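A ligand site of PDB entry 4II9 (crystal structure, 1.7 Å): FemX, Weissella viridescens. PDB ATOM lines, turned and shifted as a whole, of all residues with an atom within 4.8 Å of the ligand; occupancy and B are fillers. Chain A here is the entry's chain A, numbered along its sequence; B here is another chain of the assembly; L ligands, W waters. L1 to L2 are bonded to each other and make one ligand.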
ATOM      1  N   LYS A  37      -6.027   2.219 -13.359  1.00  0.00           N
ATOM      2  CA  LYS A  37      -6.008   2.031 -11.857  1.00  0.00           C
ATOM      3  C   LYS A  37      -6.599   3.244 -11.161  1.00  0.00           C
ATOM      4  O   LYS A  37      -5.941   3.961 -10.403  1.00  0.00           O
ATOM      5  CB  LYS A  37      -4.593   1.821 -11.336  1.00  0.00           C
ATOM      6  CG  LYS A  37      -3.854   0.666 -11.972  1.00  0.00           C
ATOM      7  CD  LYS A  37      -4.363  -0.645 -11.426  1.00  0.00           C
ATOM      8  CE  LYS A  37      -3.495  -1.840 -11.983  1.00  0.00           C
ATOM      9  NZ  LYS A  37      -4.064  -3.143 -11.499  1.00  0.00           N
ATOM     10  N   ASN A  39      -8.667   3.815  -8.830  1.00  0.00           N
ATOM     11  CA  ASN A  39      -8.782   3.783  -7.450  1.00  0.00           C
ATOM     12  C   ASN A  39      -7.467   3.989  -6.725  1.00  0.00           C
ATOM     13  O   ASN A  39      -7.439   3.884  -5.476  1.00  0.00           O
ATOM     14  CB  ASN A  39      -9.454   2.398  -7.024  1.00  0.00           C
ATOM     15  CG  ASN A  39      -8.705   1.145  -7.548  1.00  0.00           C
ATOM     16  OD1 ASN A  39      -8.205   1.170  -8.694  1.00  0.00           O
ATOM     17  ND2 ASN A  39      -8.632   0.089  -6.742  1.00  0.00           N
ATOM     18  N   TRP A  40      -6.417   4.326  -7.517  1.00  0.00           N
ATOM     19  CA  TRP A  40      -5.089   4.668  -6.914  1.00  0.00           C
ATOM     20  C   TRP A  40      -4.779   6.066  -7.257  1.00  0.00           C
ATOM     21  O   TRP A  40      -5.300   6.645  -8.233  1.00  0.00           O
ATOM     22  CB  TRP A  40      -4.004   3.746  -7.541  1.00  0.00           C
ATOM     23  CG  TRP A  40      -4.199   2.293  -7.179  1.00  0.00           C
ATOM     24  CD1 TRP A  40      -5.256   1.446  -7.591  1.00  0.00           C
ATOM     25  CD2 TRP A  40      -3.273   1.462  -6.416  1.00  0.00           C
ATOM     26  NE1 TRP A  40      -5.087   0.191  -7.017  1.00  0.00           N
ATOM     27  CE2 TRP A  40      -3.850   0.134  -6.352  1.00  0.00           C
ATOM     28  CE3 TRP A  40      -1.998   1.701  -5.824  1.00  0.00           C
ATOM     29  CZ2 TRP A  40      -3.218  -0.912  -5.653  1.00  0.00           C
ATOM     30  CZ3 TRP A  40      -1.390   0.679  -5.115  1.00  0.00           C
ATOM     31  CH2 TRP A  40      -1.969  -0.646  -5.065  1.00  0.00           C
ATOM     32  N   ASP A  64      -4.415   2.573  -0.696  1.00  0.00           N
ATOM     33  CA  ASP A  64      -4.730   2.590   0.736  1.00  0.00           C
ATOM     34  C   ASP A  64      -4.252   1.351   1.451  1.00  0.00           C
ATOM     35  O   ASP A  64      -3.976   0.230   0.852  1.00  0.00           O
ATOM     36  CB  ASP A  64      -6.231   2.841   0.936  1.00  0.00           C
ATOM     37  CG  ASP A  64      -6.593   4.286   0.725  1.00  0.00           C
ATOM     38  OD1 ASP A  64      -5.934   5.215   1.296  1.00  0.00           O
ATOM     39  OD2 ASP A  64      -7.603   4.497   0.066  1.00  0.00           O
ATOM     40  N   THR A  65      -4.107   1.527   2.773  1.00  0.00           N
ATOM     41  CA  THR A  65      -3.743   0.420   3.631  1.00  0.00           C
ATOM     42  C   THR A  65      -4.547   0.519   4.947  1.00  0.00           C
ATOM     43  O   THR A  65      -5.260   1.512   5.136  1.00  0.00           O
ATOM     44  CB  THR A  65      -2.277   0.397   4.106  1.00  0.00           C
ATOM     45  OG1 THR A  65      -2.069   1.464   5.023  1.00  0.00           O
ATOM     46  CG2 THR A  65      -1.295   0.701   2.886  1.00  0.00           C
ATOM     47  N   PHE A  71       0.574   2.915   0.364  1.00  0.00           N
ATOM     48  CA  PHE A  71       1.470   2.010  -0.274  1.00  0.00           C
ATOM     49  C   PHE A  71       1.794   2.623  -1.633  1.00  0.00           C
ATOM     50  O   PHE A  71       0.886   2.839  -2.477  1.00  0.00           O
ATOM     51  CB  PHE A  71       0.739   0.647  -0.478  1.00  0.00           C
ATOM     52  CG  PHE A  71       1.522  -0.344  -1.366  1.00  0.00           C
ATOM     53  CD1 PHE A  71       2.751  -0.833  -0.987  1.00  0.00           C
ATOM     54  CD2 PHE A  71       0.957  -0.857  -2.535  1.00  0.00           C
ATOM     55  CE1 PHE A  71       3.471  -1.710  -1.790  1.00  0.00           C
ATOM     56  CE2 PHE A  71       1.671  -1.758  -3.336  1.00  0.00           C
ATOM     57  CZ  PHE A  71       2.938  -2.175  -2.952  1.00  0.00           C
ATOM     58  N   TYR A 104       4.478   4.379   3.292  1.00  0.00           N
ATOM     59  CA  TYR A 104       5.410   3.666   4.138  1.00  0.00           C
ATOM     60  C   TYR A 104       6.532   2.997   3.358  1.00  0.00           C
ATOM     61  O   TYR A 104       7.513   2.555   3.996  1.00  0.00           O
ATOM     62  CB  TYR A 104       4.774   2.556   5.018  1.00  0.00           C
ATOM     63  CG  TYR A 104       4.253   1.311   4.302  1.00  0.00           C
ATOM     64  CD1 TYR A 104       5.007   0.109   4.310  1.00  0.00           C
ATOM     65  CD2 TYR A 104       2.997   1.310   3.647  1.00  0.00           C
ATOM     66  CE1 TYR A 104       4.556  -1.068   3.705  1.00  0.00           C
ATOM     67  CE2 TYR A 104       2.573   0.137   3.017  1.00  0.00           C
ATOM     68  CZ  TYR A 104       3.323  -1.013   3.076  1.00  0.00           C
ATOM     69  OH  TYR A 104       2.979  -2.226   2.549  1.00  0.00           O
ATOM     70  N   ARG A 107       7.671   0.676  -3.645  1.00  0.00           N
ATOM     71  CA  ARG A 107       8.045  -0.656  -4.184  1.00  0.00           C
ATOM     72  C   ARG A 107       8.107  -0.540  -5.726  1.00  0.00           C
ATOM     73  O   ARG A 107       7.234   0.066  -6.306  1.00  0.00           O
ATOM     74  CB  ARG A 107       6.918  -1.650  -3.862  1.00  0.00           C
ATOM     75  CG  ARG A 107       7.133  -3.002  -4.596  1.00  0.00           C
ATOM     76  CD  ARG A 107       6.245  -4.057  -3.966  1.00  0.00           C
ATOM     77  NE  ARG A 107       6.695  -4.400  -2.640  1.00  0.00           N
ATOM     78  CZ  ARG A 107       5.942  -4.975  -1.692  1.00  0.00           C
ATOM     79  NH1 ARG A 107       4.661  -5.416  -2.034  1.00  0.00           N
ATOM     80  NH2 ARG A 107       6.421  -5.211  -0.483  1.00  0.00           N
ATOM     81  N   ILE A 143       3.539  -9.164  -6.062  1.00  0.00           N
ATOM     82  CA  ILE A 143       2.318  -8.696  -6.692  1.00  0.00           C
ATOM     83  C   ILE A 143       2.285  -9.247  -8.126  1.00  0.00           C
ATOM     84  O   ILE A 143       1.294  -9.843  -8.517  1.00  0.00           O
ATOM     85  CB  ILE A 143       2.266  -7.161  -6.712  1.00  0.00           C
ATOM     86  CG1 ILE A 143       2.111  -6.669  -5.235  1.00  0.00           C
ATOM     87  CG2 ILE A 143       1.039  -6.701  -7.521  1.00  0.00           C
ATOM     88  CD1 ILE A 143       2.408  -5.165  -5.110  1.00  0.00           C
ATOM     89  N   THR A 210     -10.655 -15.202  -8.908  1.00  0.00           N
ATOM     90  CA  THR A 210     -11.258 -13.899  -8.949  1.00  0.00           C
ATOM     91  C   THR A 210     -11.010 -13.210 -10.305  1.00  0.00           C
ATOM     92  O   THR A 210     -10.157 -13.668 -11.112  1.00  0.00           O
ATOM     93  CB  THR A 210     -10.812 -13.021  -7.765  1.00  0.00           C
ATOM     94  OG1 THR A 210      -9.378 -12.846  -7.824  1.00  0.00           O
ATOM     95  CG2 THR A 210     -11.190 -13.705  -6.469  1.00  0.00           C
ATOM     96  N   HIS A 211     -11.801 -12.170 -10.566  1.00  0.00           N
ATOM     97  CA  HIS A 211     -11.862 -11.524 -11.922  1.00  0.00           C
ATOM     98  C   HIS A 211     -12.195 -10.084 -11.776  1.00  0.00           C
ATOM     99  O   HIS A 211     -12.888  -9.679 -10.801  1.00  0.00           O
ATOM    100  CB  HIS A 211     -12.911 -12.254 -12.823  1.00  0.00           C
ATOM    101  CG  HIS A 211     -14.290 -12.427 -12.136  1.00  0.00           C
ATOM    102  ND1 HIS A 211     -14.525 -13.357 -11.195  1.00  0.00           N
ATOM    103  CD2 HIS A 211     -15.461 -11.691 -12.286  1.00  0.00           C
ATOM    104  CE1 HIS A 211     -15.827 -13.184 -10.700  1.00  0.00           C
ATOM    105  NE2 HIS A 211     -16.370 -12.180 -11.409  1.00  0.00           N
ATOM    106  N   ARG A 212     -11.737  -9.252 -12.718  1.00  0.00           N
ATOM    107  CA  ARG A 212     -11.942  -7.816 -12.615  1.00  0.00           C
ATOM    108  C   ARG A 212     -13.267  -7.421 -13.308  1.00  0.00           C
ATOM    109  O   ARG A 212     -13.728  -8.138 -14.238  1.00  0.00           O
ATOM    110  CB  ARG A 212     -10.801  -7.155 -13.415  1.00  0.00           C
ATOM    111  CG  ARG A 212      -9.470  -7.517 -12.706  1.00  0.00           C
ATOM    112  CD  ARG A 212      -8.367  -6.645 -13.383  1.00  0.00           C
ATOM    113  NE  ARG A 212      -6.980  -6.895 -12.816  1.00  0.00           N
ATOM    114  CZ  ARG A 212      -6.497  -6.189 -11.789  1.00  0.00           C
ATOM    115  NH1 ARG A 212      -7.279  -5.365 -11.094  1.00  0.00           N
ATOM    116  NH2 ARG A 212      -5.254  -6.473 -11.386  1.00  0.00           N
ATOM    117  N   PRO A 213     -13.851  -6.279 -12.973  1.00  0.00           N
ATOM    118  CA  PRO A 213     -15.139  -5.869 -13.572  1.00  0.00           C
ATOM    119  C   PRO A 213     -14.897  -5.328 -14.960  1.00  0.00           C
ATOM    120  O   PRO A 213     -13.742  -4.968 -15.295  1.00  0.00           O
ATOM    121  CB  PRO A 213     -15.638  -4.693 -12.648  1.00  0.00           C
ATOM    122  CG  PRO A 213     -14.665  -4.592 -11.580  1.00  0.00           C
ATOM    123  CD  PRO A 213     -13.478  -5.417 -11.827  1.00  0.00           C
ATOM    124  N   TYR A 216     -12.876  -2.034 -15.805  1.00  0.00           N
ATOM    125  CA  TYR A 216     -11.330  -2.008 -15.758  1.00  0.00           C
ATOM    126  C   TYR A 216     -10.845  -2.010 -17.198  1.00  0.00           C
ATOM    127  O   TYR A 216      -9.987  -1.203 -17.588  1.00  0.00           O
ATOM    128  CB  TYR A 216     -10.884  -3.240 -15.036  1.00  0.00           C
ATOM    129  CG  TYR A 216      -9.396  -3.335 -14.784  1.00  0.00           C
ATOM    130  CD1 TYR A 216      -8.813  -2.725 -13.657  1.00  0.00           C
ATOM    131  CD2 TYR A 216      -8.598  -3.956 -15.730  1.00  0.00           C
ATOM    132  CE1 TYR A 216      -7.425  -2.886 -13.415  1.00  0.00           C
ATOM    133  CE2 TYR A 216      -7.204  -4.157 -15.499  1.00  0.00           C
ATOM    134  CZ  TYR A 216      -6.684  -3.557 -14.320  1.00  0.00           C
ATOM    135  OH  TYR A 216      -5.358  -3.658 -13.963  1.00  0.00           O
ATOM    136  N   LEU A 333       3.163  -4.633   7.817  1.00  0.00           N
ATOM    137  CA  LEU A 333       2.441  -4.965   6.558  1.00  0.00           C
ATOM    138  C   LEU A 333       3.190  -5.910   5.621  1.00  0.00           C
ATOM    139  O   LEU A 333       2.517  -6.457   4.733  1.00  0.00           O
ATOM    140  CB  LEU A 333       2.089  -3.727   5.764  1.00  0.00           C
ATOM    141  CG  LEU A 333       1.142  -2.759   6.516  1.00  0.00           C
ATOM    142  CD1 LEU A 333       0.755  -1.613   5.613  1.00  0.00           C
ATOM    143  CD2 LEU A 333      -0.085  -3.537   7.060  1.00  0.00           C
ATOM    144  N   ALA B   1      -7.146 -10.615  -7.138  1.00  0.00           N
ATOM    145  CA  ALA B   1      -6.193 -11.397  -6.322  1.00  0.00           C
ATOM    146  C   ALA B   1      -5.720 -12.704  -6.943  1.00  0.00           C
ATOM    147  O   ALA B   1      -4.576 -13.191  -6.691  1.00  0.00           O
ATOM    148  CB  ALA B   1      -6.902 -11.671  -4.981  1.00  0.00           C
ATOM    149  N   FGA B   2      -6.557 -13.296  -7.817  1.00  0.00           N
ATOM    150  CA  FGA B   2      -6.178 -14.518  -8.498  1.00  0.00           C
ATOM    151  C   FGA B   2      -6.936 -15.750  -7.928  1.00  0.00           C
ATOM    152  O   FGA B   2      -8.110 -15.607  -7.438  1.00  0.00           O
ATOM    153  CB  FGA B   2      -6.508 -14.422 -10.006  1.00  0.00           C
ATOM    154  CG  FGA B   2      -5.785 -13.273 -10.770  1.00  0.00           C
ATOM    155  CD  FGA B   2      -4.324 -13.601 -11.007  1.00  0.00           C
ATOM    156  OE1 FGA B   2      -3.731 -14.524 -10.468  1.00  0.00           O
ATOM    157  OXT FGA B   2      -6.380 -16.880  -8.018  1.00  0.00           O
ATOM    158  N   CYS B   3      -3.687 -12.499 -11.608  1.00  0.00           N
ATOM    159  CA  CYS B   3      -2.270 -12.726 -12.084  1.00  0.00           C
ATOM    160  C   CYS B   3      -1.657 -11.317 -12.146  1.00  0.00           C
ATOM    161  O   CYS B   3      -1.011 -10.962 -13.143  1.00  0.00           O
ATOM    162  CB  CYS B   3      -2.376 -13.441 -13.529  1.00  0.00           C
ATOM    163  SG  CYS B   3      -1.148 -14.765 -13.428  1.00  0.00           S
ATOM    164  N   DAL B   4      -1.875 -10.479 -11.114  1.00  0.00           N
ATOM    165  CA  DAL B   4      -1.411  -9.085 -11.260  1.00  0.00           C
ATOM    166  CB  DAL B   4      -1.637  -8.321  -9.957  1.00  0.00           C
ATOM    167  C   DAL B   4      -2.038  -8.290 -12.368  1.00  0.00           C
ATOM    168  O   DAL B   4      -3.274  -8.357 -12.564  1.00  0.00           O
ATOM    169  N   DAL B   5      -1.195  -7.554 -13.131  1.00  0.00           N
ATOM    170  CA  DAL B   5      -1.716  -6.874 -14.324  1.00  0.00           C
ATOM    171  CB  DAL B   5      -0.571  -6.122 -15.004  1.00  0.00           C
ATOM    172  C   DAL B   5      -2.826  -5.851 -13.947  1.00  0.00           C
ATOM    173  O   DAL B   5      -3.847  -5.617 -14.665  1.00  0.00           O
ATOM    174  OXT DAL B   5      -2.744  -5.173 -12.894  1.00  0.00           O
HETATM  175  C1  LIG L   1      -7.354  -5.254  -6.703  1.00  0.00           C
HETATM  176  C2  LIG L   1      -7.363  -6.755  -6.909  1.00  0.00           C
HETATM  177  C3  LIG L   1      -8.371  -7.070  -8.029  1.00  0.00           C
HETATM  178  C4  LIG L   1      -9.744  -6.426  -7.728  1.00  0.00           C
HETATM  179  C5  LIG L   1      -9.593  -4.936  -7.459  1.00  0.00           C
HETATM  180  C6  LIG L   1     -10.889  -4.452  -6.828  1.00  0.00           C
HETATM  181  C7  LIG L   1      -5.198  -7.909  -6.442  1.00  0.00           C
HETATM  182  C8  LIG L   1      -3.825  -8.327  -6.904  1.00  0.00           C
HETATM  183  C9  LIG L   1      -7.722  -9.196  -9.064  1.00  0.00           C
HETATM  184  C10 LIG L   1      -6.759 -10.094  -8.354  1.00  0.00           C
HETATM  185  C11 LIG L   1      -8.696 -10.034  -9.939  1.00  0.00           C
HETATM  186  O1  LIG L   1      -6.951  -4.662  -7.924  1.00  0.00           O
HETATM  187  O2  LIG L   1      -8.528  -8.481  -8.114  1.00  0.00           O
HETATM  188  O3  LIG L   1     -10.594  -6.570  -8.887  1.00  0.00           O
HETATM  189  O4  LIG L   1      -8.657  -4.751  -6.392  1.00  0.00           O
HETATM  190  O5  LIG L   1     -10.924  -3.015  -6.862  1.00  0.00           O
HETATM  191  O6  LIG L   1      -5.612  -8.307  -5.352  1.00  0.00           O
HETATM  192  O7  LIG L   1      -5.665 -10.282  -8.910  1.00  0.00           O
HETATM  193  N1  LIG L   1      -5.990  -7.209  -7.247  1.00  0.00           N
HETATM  194  N1  LG2 L   2      -0.415  -4.342  -1.799  1.00  0.00           N
HETATM  195  C1  LG2 L   2       0.777  -4.616  -1.082  1.00  0.00           C
HETATM  196  N2  LG2 L   2       1.093  -3.844   0.034  1.00  0.00           N
HETATM  197  C2  LG2 L   2       0.205  -2.911   0.404  1.00  0.00           C
HETATM  198  C3  LG2 L   2      -0.968  -2.633  -0.315  1.00  0.00           C
HETATM  199  C4  LG2 L   2      -1.255  -3.355  -1.459  1.00  0.00           C
HETATM  200  O1  LG2 L   2       1.576  -5.458  -1.458  1.00  0.00           O
HETATM  201  O2  LG2 L   2       0.445  -2.201   1.463  1.00  0.00           O
HETATM  202  C5  LG2 L   2      -0.704  -5.225  -2.957  1.00  0.00           C
HETATM  203  C6  LG2 L   2      -2.086  -5.802  -2.845  1.00  0.00           C
HETATM  204  O3  LG2 L   2      -2.089  -6.902  -1.958  1.00  0.00           O
HETATM  205  C7  LG2 L   2      -2.361  -6.303  -4.250  1.00  0.00           C
HETATM  206  C8  LG2 L   2      -1.552  -5.306  -5.055  1.00  0.00           C
HETATM  207  O4  LG2 L   2      -0.899  -4.451  -4.087  1.00  0.00           O
HETATM  208  O5  LG2 L   2      -1.680  -7.517  -4.567  1.00  0.00           O
HETATM  209  C9  LG2 L   2      -2.372  -4.371  -5.887  1.00  0.00           C
HETATM  210  O6  LG2 L   2      -3.036  -5.159  -6.938  1.00  0.00           O
HETATM  211  P1  LG2 L   2      -3.585  -4.532  -8.194  1.00  0.00           P
HETATM  212  O7  LG2 L   2      -2.646  -3.659  -8.964  1.00  0.00           O
HETATM  213  O8  LG2 L   2      -4.246  -5.630  -9.003  1.00  0.00           O
HETATM  214  O9  LG2 L   2      -4.719  -3.564  -7.568  1.00  0.00           O
HETATM  215  P2  LG2 L   2      -6.175  -3.253  -8.101  1.00  0.00           P
HETATM  216  O10 LG2 L   2      -6.115  -2.975  -9.561  1.00  0.00           O
HETATM  217  O11 LG2 L   2      -6.743  -2.181  -7.143  1.00  0.00           O
HETATM  218  O   HOH W   1     -10.025  -4.798 -11.051  1.00  0.00           O
HETATM  219  O   HOH W   2     -10.407  -1.904  -9.769  1.00  0.00           O
HETATM  220  O   HOH W   3      -5.195 -10.001 -11.642  1.00  0.00           O
HETATM  221  O   HOH W   4      -9.843  -2.669  -4.396  1.00  0.00           O
HETATM  222  O   HOH W   5      -1.596  -1.120  -8.646  1.00  0.00           O
HETATM  223  O   HOH W   6     -12.359  -8.331  -8.540  1.00  0.00           O
HETATM  224  O   HOH W   7      -7.994  -1.012 -10.305  1.00  0.00           O
HETATM  225  O   HOH W   8      -3.718  -9.553  -3.919  1.00  0.00           O
HETATM  226  O   HOH W   9      -4.524  -3.284  -1.061  1.00  0.00           O
HETATM  227  O   HOH W  10       2.250  -6.257   1.954  1.00  0.00           O
HETATM  228  O   HOH W  11      -1.045  -4.782 -10.898  1.00  0.00           O
HETATM  229  O   HOH W  12      -2.858 -11.318  -8.646  1.00  0.00           O
HETATM  230  O   HOH W  13      -6.861  -2.370  -4.508  1.00  0.00           O
HETATM  231  O   HOH W  14       1.891  -8.175  -1.386  1.00  0.00           O
HETATM  232  O   HOH W  15      -1.783  -2.787   3.157  1.00  0.00           O
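The side-chain hydroxyl of Thr 210 sits at hydrogen-bond distance from the backbone NH of Ala 1 of chain B, at 3.2 Å.
O of DAL 4 of chain B sits at hydrogen-bond distance from the guanidinium group (NH2) of Arg 212, at 3.0 Å.
NH2 of Arg 212 is in salt-bridge range of OXT of DAL 5 of chain B.
NZ of Lys 37 sits at hydrogen-bond distance from OH of Tyr 216 (2.8 Å).
NZ of Lys 37 is in salt-bridge range of OXT of DAL 5 of chain B (2.8 Å).
N of FGA 2 of chain B sits at hydrogen-bond distance from OG1 of Thr 210 (2.9 Å).
Thr 65 touches the ligand.
Phe 71 touches the ligand.
Ile 143 touches the ligand.
OG1 of Thr 210 touches C11 of LIG L1, 3.6 Å away.
His 211 touches the ligand.
CB of DAL 4 of chain B touches C8 of LIG L1 (3.8 Å).
Hydrophobic or aromatic side chains that line the ligand: Trp 40, Phe 71, Tyr 104, Ile 143 and Ala 1 of chain B.
Water W6 lies within hydrogen-bond range of O3 of LIG L1 (2.5 Å) and O of His 211 (2.7 Å).
Water W11 lies within hydrogen-bond range of OXT of DAL 5 of chain B (2.7 Å), O7 of LG2 L2 (2.8 Å) and NZ of Lys 37 (3.5 Å).
Water W3 lies within hydrogen-bond range of O of DAL 4 of chain B (2.7 Å), an oxygen (O7) of LIG L1 (2.8 Å) and the backbone NH of Cys 3 of chain B (2.9 Å).
Water W1 bridges the guanidinium group (NH1) of Arg 212 (2.8 Å) and an oxygen (O3) of LIG L1 (2.9 Å).
Water W12 lies within hydrogen-bond range of N of DAL 4 of chain B (2.8 Å), O7 of LIG L1 (3.0 Å), O of Ala 1 of chain B (3.2 Å) and N of Cys 3 of chain B (3.3 Å).
Water W10 lies within hydrogen-bond range of O of Leu 333 (2.8 Å) and N2 of LG2 L2 (3.3 Å).
N of Ala 1 of chain B is bonded to C10 of LIG L1, 1.4 Å away.
The guanidinium group (NH2) of Arg 212 lies within salt-bridge range of an oxygen (O8) of LG2 L2, at 2.7 Å.
The side-chain hydroxyl (OH) of Tyr 104 is in hydrogen-bond range of an oxygen (O2) of LG2 L2 (2.8 Å).
The side-chain amino group of Lys 37 lies within salt-bridge range of an oxygen (O10) of LG2 L2 (2.8 Å).
The indole nitrogen (NE1) of Trp 40 lies within hydrogen-bond range of an oxygen (O11) of LG2 L2 (2.9 Å).
ND2 of Asn 39 sits at hydrogen-bond distance from O11 of LG2 L2 (3.0 Å).
NH1 of Arg 107 lies within hydrogen-bond range of O1 of LG2 L2 (3.1 Å).
An oxygen (O7) of LIG L1 sits close to N of FGA 2 of chain B (3.3 Å).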
